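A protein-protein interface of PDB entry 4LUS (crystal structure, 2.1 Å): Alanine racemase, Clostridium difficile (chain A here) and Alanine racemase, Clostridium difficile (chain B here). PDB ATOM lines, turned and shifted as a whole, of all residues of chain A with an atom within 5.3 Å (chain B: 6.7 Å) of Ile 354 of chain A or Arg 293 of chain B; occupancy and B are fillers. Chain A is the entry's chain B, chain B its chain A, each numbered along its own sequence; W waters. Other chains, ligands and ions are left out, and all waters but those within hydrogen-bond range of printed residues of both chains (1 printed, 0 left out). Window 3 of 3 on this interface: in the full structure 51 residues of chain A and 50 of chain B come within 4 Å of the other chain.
Water W1 bridges the backbone carbonyl oxygen (O) of Tyr 287 of chain B (2.6 Å) and the side-chain carboxylate (OE2) of Glu 357 of chain A (2.9 Å).
Thr 353 of chain A touches Arg 293 of chain B.
Ile 354 of chain A touches Tyr 287 of chain B (CD1 to OH, 3.8 Å).
NE of Arg 293 of chain B touches CD1 of Ile 354 of chain A (3.9 Å).
Tyr 356 of chain A touches Tyr 287 of chain B (CB to OH, 3.4 Å).
Tyr 287 of chain B touches Glu 357 of chain A.
Ile 294 of chain B touches Glu 357 of chain A (CG1 to OE1, 3.96 Å).
OG1 of Thr 292 of chain B lies within hydrogen-bond range of OE2 of Glu 357 of chain A (2.9 Å).
N of Arg 293 of chain B is in hydrogen-bond range of OE2 of Glu 357 of chain A, 3.2 Å away.
Of the 14 printed residues of chain B, 4 touch a printed residue of chain A.
Printed residues of chain B that touch a printed residue of chain A: Tyr 287, Thr 292, Arg 293 and Ile 294.
Hydrophobic or aromatic side chains of chain B that line the printed part of chain A: Tyr 287 and Ile 294.
Hydrophobic or aromatic side chains of chain A within 4 Å of the printed part of chain B: Ile 354 and Tyr 356.
Among the printed residues, 8 pairs touch across the chains.
Among the printed residues, no Asp or Glu carboxylate lies within 4 Å of a Lys or Arg side-chain nitrogen of the other chain.
Printed residues of chain B within 4 Å of Thr 353 of chain A: Arg 293 (3.6 Å).
Of chain B, only Tyr 287 (3.8 Å) and Arg 293 (3.9 Å) come within 4 Å of Ile 354 of chain A.
Of the printed residues of chain B, Tyr 356 of chain A touches Tyr 287 (3.4 Å).
Of the printed residues of chain A, Ile 294 of chain B touches Glu 357 (3.96 Å).
Pro 298 of chain B touches none of the printed residues of chain A.
The nearest residue of chain B that does not touch Ile 354 of chain A is Arg 312 of chain B (6.3 Å).
OG1 of Thr 292 of chain B lies close to N of Ile 294 of chain B, at 3.2 Å.
The side-chain amide nitrogen (NE2) of Gln 295 of chain B lies within hydrogen-bond range of the backbone carbonyl oxygen (O) of Thr 292 of chain B (2.8 Å).
The backbone carbonyl oxygen (O) of Ala 348 of chain A is in hydrogen-bond range of the backbone NH (N) of Thr 353 of chain A.
The side-chain carboxylate of Glu 357 of chain A is in hydrogen-bond range of the side-chain hydroxyl of Thr 353 of chain A.
O of Cys 314 of chain B is in hydrogen-bond range of N of Tyr 287 of chain B (3.0 Å).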
ATOM      1  N   ALA A 348       2.280   3.555  29.030  1.00  0.00           N
ATOM      2  CA  ALA A 348       2.665   4.345  27.893  1.00  0.00           C
ATOM      3  C   ALA A 348       4.182   4.294  27.634  1.00  0.00           C
ATOM      4  O   ALA A 348       4.579   4.116  26.560  1.00  0.00           O
ATOM      5  CB  ALA A 348       2.221   5.784  28.073  1.00  0.00           C
ATOM      6  N   GLY A 352       6.108   2.787  24.321  1.00  0.00           N
ATOM      7  CA  GLY A 352       6.560   3.886  23.518  1.00  0.00           C
ATOM      8  C   GLY A 352       5.519   4.758  22.872  1.00  0.00           C
ATOM      9  O   GLY A 352       5.603   5.013  21.739  1.00  0.00           O
ATOM     10  N   THR A 353       4.535   5.180  23.652  1.00  0.00           N
ATOM     11  CA  THR A 353       3.496   6.107  23.291  1.00  0.00           C
ATOM     12  C   THR A 353       3.291   7.022  24.460  1.00  0.00           C
ATOM     13  O   THR A 353       4.131   7.130  25.281  1.00  0.00           O
ATOM     14  CB  THR A 353       2.142   5.457  22.858  1.00  0.00           C
ATOM     15  OG1 THR A 353       1.233   6.470  22.510  1.00  0.00           O
ATOM     16  CG2 THR A 353       1.504   4.630  23.959  1.00  0.00           C
ATOM     17  N   ILE A 354       2.139   7.656  24.526  1.00  0.00           N
ATOM     18  CA  ILE A 354       1.859   8.671  25.505  1.00  0.00           C
ATOM     19  C   ILE A 354       0.626   8.389  26.312  1.00  0.00           C
ATOM     20  O   ILE A 354      -0.203   7.700  25.886  1.00  0.00           O
ATOM     21  CB  ILE A 354       1.690  10.018  24.860  1.00  0.00           C
ATOM     22  CG1 ILE A 354       0.716   9.924  23.724  1.00  0.00           C
ATOM     23  CG2 ILE A 354       2.999  10.519  24.340  1.00  0.00           C
ATOM     24  CD1 ILE A 354       0.383  11.243  23.120  1.00  0.00           C
ATOM     25  N   ASN A 355       0.489   9.039  27.435  1.00  0.00           N
ATOM     26  CA  ASN A 355      -0.603   8.783  28.318  1.00  0.00           C
ATOM     27  C   ASN A 355      -1.972   8.966  27.668  1.00  0.00           C
ATOM     28  O   ASN A 355      -2.830   8.198  27.916  1.00  0.00           O
ATOM     29  CB  ASN A 355      -0.489   9.565  29.615  1.00  0.00           C
ATOM     30  CG  ASN A 355      -0.199  11.042  29.421  1.00  0.00           C
ATOM     31  OD1 ASN A 355      -0.272  11.587  28.367  1.00  0.00           O
ATOM     32  ND2 ASN A 355       0.108  11.657  30.471  1.00  0.00           N
ATOM     33  N   TYR A 356      -2.098   9.922  26.775  1.00  0.00           N
ATOM     34  CA  TYR A 356      -3.338  10.235  26.140  1.00  0.00           C
ATOM     35  C   TYR A 356      -3.850   9.013  25.424  1.00  0.00           C
ATOM     36  O   TYR A 356      -5.005   8.759  25.433  1.00  0.00           O
ATOM     37  CB  TYR A 356      -3.174  11.277  25.062  1.00  0.00           C
ATOM     38  CG  TYR A 356      -2.689  12.639  25.403  1.00  0.00           C
ATOM     39  CD1 TYR A 356      -1.389  12.872  25.691  1.00  0.00           C
ATOM     40  CD2 TYR A 356      -3.520  13.703  25.325  1.00  0.00           C
ATOM     41  CE1 TYR A 356      -0.949  14.127  25.966  1.00  0.00           C
ATOM     42  CE2 TYR A 356      -3.090  14.960  25.584  1.00  0.00           C
ATOM     43  CZ  TYR A 356      -1.808  15.163  25.896  1.00  0.00           C
ATOM     44  OH  TYR A 356      -1.417  16.377  26.165  1.00  0.00           O
ATOM     45  N   GLU A 357      -2.972   8.290  24.768  1.00  0.00           N
ATOM     46  CA  GLU A 357      -3.362   7.110  24.062  1.00  0.00           C
ATOM     47  C   GLU A 357      -3.863   5.966  24.917  1.00  0.00           C
ATOM     48  O   GLU A 357      -4.798   5.348  24.577  1.00  0.00           O
ATOM     49  CB  GLU A 357      -2.329   6.645  23.072  1.00  0.00           C
ATOM     50  CG  GLU A 357      -2.941   5.646  22.121  1.00  0.00           C
ATOM     51  CD  GLU A 357      -2.010   5.026  21.121  1.00  0.00           C
ATOM     52  OE1 GLU A 357      -0.837   4.947  21.352  1.00  0.00           O
ATOM     53  OE2 GLU A 357      -2.479   4.624  20.107  1.00  0.00           O
ATOM     54  N   VAL A 358      -3.215   5.718  26.025  1.00  0.00           N
ATOM     55  CA  VAL A 358      -3.635   4.686  26.919  1.00  0.00           C
ATOM     56  C   VAL A 358      -5.037   4.969  27.441  1.00  0.00           C
ATOM     57  O   VAL A 358      -5.811   4.090  27.591  1.00  0.00           O
ATOM     58  CB  VAL A 358      -2.657   4.551  28.063  1.00  0.00           C
ATOM     59  CG1 VAL A 358      -3.141   3.552  29.062  1.00  0.00           C
ATOM     60  CG2 VAL A 358      -1.302   4.189  27.537  1.00  0.00           C
ATOM     61  N   GLY B 286      -7.440   9.244  13.593  1.00  0.00           N
ATOM     62  CA  GLY B 286      -6.361   9.244  14.538  1.00  0.00           C
ATOM     63  C   GLY B 286      -6.340   8.094  15.520  1.00  0.00           C
ATOM     64  O   GLY B 286      -7.111   7.196  15.422  1.00  0.00           O
ATOM     65  N   TYR B 287      -5.458   8.183  16.496  1.00  0.00           N
ATOM     66  CA  TYR B 287      -5.299   7.136  17.468  1.00  0.00           C
ATOM     67  C   TYR B 287      -6.532   6.888  18.297  1.00  0.00           C
ATOM     68  O   TYR B 287      -6.748   5.823  18.718  1.00  0.00           O
ATOM     69  CB  TYR B 287      -4.004   7.202  18.282  1.00  0.00           C
ATOM     70  CG  TYR B 287      -3.777   8.380  19.168  1.00  0.00           C
ATOM     71  CD1 TYR B 287      -4.488   8.543  20.308  1.00  0.00           C
ATOM     72  CD2 TYR B 287      -2.786   9.284  18.903  1.00  0.00           C
ATOM     73  CE1 TYR B 287      -4.269   9.593  21.139  1.00  0.00           C
ATOM     74  CE2 TYR B 287      -2.576  10.334  19.722  1.00  0.00           C
ATOM     75  CZ  TYR B 287      -3.348  10.497  20.838  1.00  0.00           C
ATOM     76  OH  TYR B 287      -3.170  11.511  21.668  1.00  0.00           O
ATOM     77  N   GLY B 290      -8.670   4.280  17.123  1.00  0.00           N
ATOM     78  CA  GLY B 290      -7.956   3.041  17.097  1.00  0.00           C
ATOM     79  C   GLY B 290      -6.945   2.826  15.992  1.00  0.00           C
ATOM     80  O   GLY B 290      -6.594   1.727  15.721  1.00  0.00           O
ATOM     81  N   PHE B 291      -6.508   3.873  15.340  1.00  0.00           N
ATOM     82  CA  PHE B 291      -5.423   3.760  14.420  1.00  0.00           C
ATOM     83  C   PHE B 291      -4.195   4.144  15.198  1.00  0.00           C
ATOM     84  O   PHE B 291      -3.880   5.283  15.324  1.00  0.00           O
ATOM     85  CB  PHE B 291      -5.660   4.703  13.295  1.00  0.00           C
ATOM     86  CG  PHE B 291      -4.693   4.606  12.173  1.00  0.00           C
ATOM     87  CD1 PHE B 291      -4.726   3.533  11.306  1.00  0.00           C
ATOM     88  CD2 PHE B 291      -3.820   5.616  11.932  1.00  0.00           C
ATOM     89  CE1 PHE B 291      -3.876   3.459  10.251  1.00  0.00           C
ATOM     90  CE2 PHE B 291      -2.979   5.556  10.875  1.00  0.00           C
ATOM     91  CZ  PHE B 291      -3.003   4.480  10.036  1.00  0.00           C
ATOM     92  N   THR B 292      -3.528   3.164  15.755  1.00  0.00           N
ATOM     93  CA  THR B 292      -2.603   3.402  16.803  1.00  0.00           C
ATOM     94  C   THR B 292      -1.352   4.183  16.433  1.00  0.00           C
ATOM     95  O   THR B 292      -0.800   4.033  15.425  1.00  0.00           O
ATOM     96  CB  THR B 292      -2.294   2.138  17.568  1.00  0.00           C
ATOM     97  OG1 THR B 292      -1.362   2.427  18.559  1.00  0.00           O
ATOM     98  CG2 THR B 292      -1.723   1.129  16.677  1.00  0.00           C
ATOM     99  N   ARG B 293      -0.982   5.038  17.338  1.00  0.00           N
ATOM    100  CA  ARG B 293       0.162   5.897  17.275  1.00  0.00           C
ATOM    101  C   ARG B 293       1.446   5.111  17.265  1.00  0.00           C
ATOM    102  O   ARG B 293       2.432   5.561  16.848  1.00  0.00           O
ATOM    103  CB  ARG B 293       0.138   6.799  18.480  1.00  0.00           C
ATOM    104  CG  ARG B 293       0.899   8.082  18.356  1.00  0.00           C
ATOM    105  CD  ARG B 293       1.062   8.678  19.726  1.00  0.00           C
ATOM    106  NE  ARG B 293       1.747   9.944  19.720  1.00  0.00           N
ATOM    107  CZ  ARG B 293       2.947  10.164  20.201  1.00  0.00           C
ATOM    108  NH1 ARG B 293       3.682   9.230  20.735  1.00  0.00           N
ATOM    109  NH2 ARG B 293       3.426  11.353  20.141  1.00  0.00           N
ATOM    110  N   ILE B 294       1.384   3.909  17.767  1.00  0.00           N
ATOM    111  CA  ILE B 294       2.553   3.081  17.914  1.00  0.00           C
ATOM    112  C   ILE B 294       3.200   2.702  16.597  1.00  0.00           C
ATOM    113  O   ILE B 294       4.322   2.402  16.553  1.00  0.00           O
ATOM    114  CB  ILE B 294       2.266   1.865  18.785  1.00  0.00           C
ATOM    115  CG1 ILE B 294       1.910   2.348  20.166  1.00  0.00           C
ATOM    116  CG2 ILE B 294       3.463   0.956  18.845  1.00  0.00           C
ATOM    117  CD1 ILE B 294       1.155   1.398  20.978  1.00  0.00           C
ATOM    118  N   GLN B 295       2.434   2.755  15.544  1.00  0.00           N
ATOM    119  CA  GLN B 295       2.852   2.382  14.250  1.00  0.00           C
ATOM    120  C   GLN B 295       4.087   3.154  13.797  1.00  0.00           C
ATOM    121  O   GLN B 295       4.132   4.325  13.869  1.00  0.00           O
ATOM    122  CB  GLN B 295       1.709   2.689  13.306  1.00  0.00           C
ATOM    123  CG  GLN B 295       0.537   1.786  13.450  1.00  0.00           C
ATOM    124  CD  GLN B 295      -0.601   2.127  12.541  1.00  0.00           C
ATOM    125  OE1 GLN B 295      -0.691   1.627  11.495  1.00  0.00           O
ATOM    126  NE2 GLN B 295      -1.469   2.944  12.982  1.00  0.00           N
ATOM    127  N   LYS B 296       5.091   2.435  13.374  1.00  0.00           N
ATOM    128  CA  LYS B 296       6.252   3.043  12.785  1.00  0.00           C
ATOM    129  C   LYS B 296       6.190   3.169  11.288  1.00  0.00           C
ATOM    130  O   LYS B 296       6.802   4.011  10.794  1.00  0.00           O
ATOM    131  CB  LYS B 296       7.536   2.343  13.189  1.00  0.00           C
ATOM    132  CG  LYS B 296       7.972   2.511  14.615  1.00  0.00           C
ATOM    133  CD  LYS B 296       9.052   1.499  14.915  1.00  0.00           C
ATOM    134  CE  LYS B 296       9.606   1.598  16.307  1.00  0.00           C
ATOM    135  NZ  LYS B 296      10.926   2.229  16.379  1.00  0.00           N
ATOM    136  N   PRO B 298       3.108   3.515   9.199  1.00  0.00           N
ATOM    137  CA  PRO B 298       1.721   3.614   8.792  1.00  0.00           C
ATOM    138  C   PRO B 298       1.534   3.995   7.343  1.00  0.00           C
ATOM    139  O   PRO B 298       2.182   4.886   6.902  1.00  0.00           O
ATOM    140  CB  PRO B 298       1.173   4.699   9.691  1.00  0.00           C
ATOM    141  CG  PRO B 298       2.313   5.351  10.321  1.00  0.00           C
ATOM    142  CD  PRO B 298       3.549   4.784   9.759  1.00  0.00           C
ATOM    143  N   ARG B 312       3.931  12.170  13.464  1.00  0.00           N
ATOM    144  CA  ARG B 312       3.233  11.440  14.470  1.00  0.00           C
ATOM    145  C   ARG B 312       1.775  11.341  14.149  1.00  0.00           C
ATOM    146  O   ARG B 312       1.187  12.274  13.695  1.00  0.00           O
ATOM    147  CB  ARG B 312       3.408  12.146  15.792  1.00  0.00           C
ATOM    148  CG  ARG B 312       4.516  11.609  16.651  1.00  0.00           C
ATOM    149  CD  ARG B 312       5.217  12.733  17.356  1.00  0.00           C
ATOM    150  NE  ARG B 312       6.389  12.288  18.087  1.00  0.00           N
ATOM    151  CZ  ARG B 312       6.764  12.765  19.268  1.00  0.00           C
ATOM    152  NH1 ARG B 312       6.064  13.708  19.863  1.00  0.00           N
ATOM    153  NH2 ARG B 312       7.842  12.295  19.857  1.00  0.00           N
ATOM    154  N   ILE B 313       1.192  10.199  14.412  1.00  0.00           N
ATOM    155  CA  ILE B 313      -0.242  10.049  14.396  1.00  0.00           C
ATOM    156  C   ILE B 313      -0.858  10.872  15.514  1.00  0.00           C
ATOM    157  O   ILE B 313      -0.436  10.788  16.624  1.00  0.00           O
ATOM    158  CB  ILE B 313      -0.632   8.580  14.479  1.00  0.00           C
ATOM    159  CG1 ILE B 313      -0.278   7.932  13.163  1.00  0.00           C
ATOM    160  CG2 ILE B 313      -2.100   8.411  14.781  1.00  0.00           C
ATOM    161  CD1 ILE B 313      -0.215   6.441  13.144  1.00  0.00           C
ATOM    162  N   CYS B 314      -1.832  11.695  15.169  1.00  0.00           N
ATOM    163  CA  CYS B 314      -2.535  12.483  16.145  1.00  0.00           C
ATOM    164  C   CYS B 314      -3.778  11.819  16.705  1.00  0.00           C
ATOM    165  O   CYS B 314      -4.227  10.869  16.186  1.00  0.00           O
ATOM    166  CB  CYS B 314      -2.825  13.874  15.619  1.00  0.00           C
ATOM    167  SG  CYS B 314      -1.357  14.847  15.273  1.00  0.00           S
ATOM    168  N   LEU B 351       3.413  -3.492  14.158  1.00  0.00           N
ATOM    169  CA  LEU B 351       3.259  -3.276  15.576  1.00  0.00           C
ATOM    170  C   LEU B 351       3.832  -4.399  16.483  1.00  0.00           C
ATOM    171  O   LEU B 351       3.986  -4.236  17.645  1.00  0.00           O
ATOM    172  CB  LEU B 351       1.776  -3.060  15.872  1.00  0.00           C
ATOM    173  CG  LEU B 351       1.057  -1.827  15.368  1.00  0.00           C
ATOM    174  CD1 LEU B 351      -0.399  -1.972  15.544  1.00  0.00           C
ATOM    175  CD2 LEU B 351       1.547  -0.525  15.917  1.00  0.00           C
HETATM  176  O   HOH W   1      -5.179   3.859  19.495  1.00  0.00           O
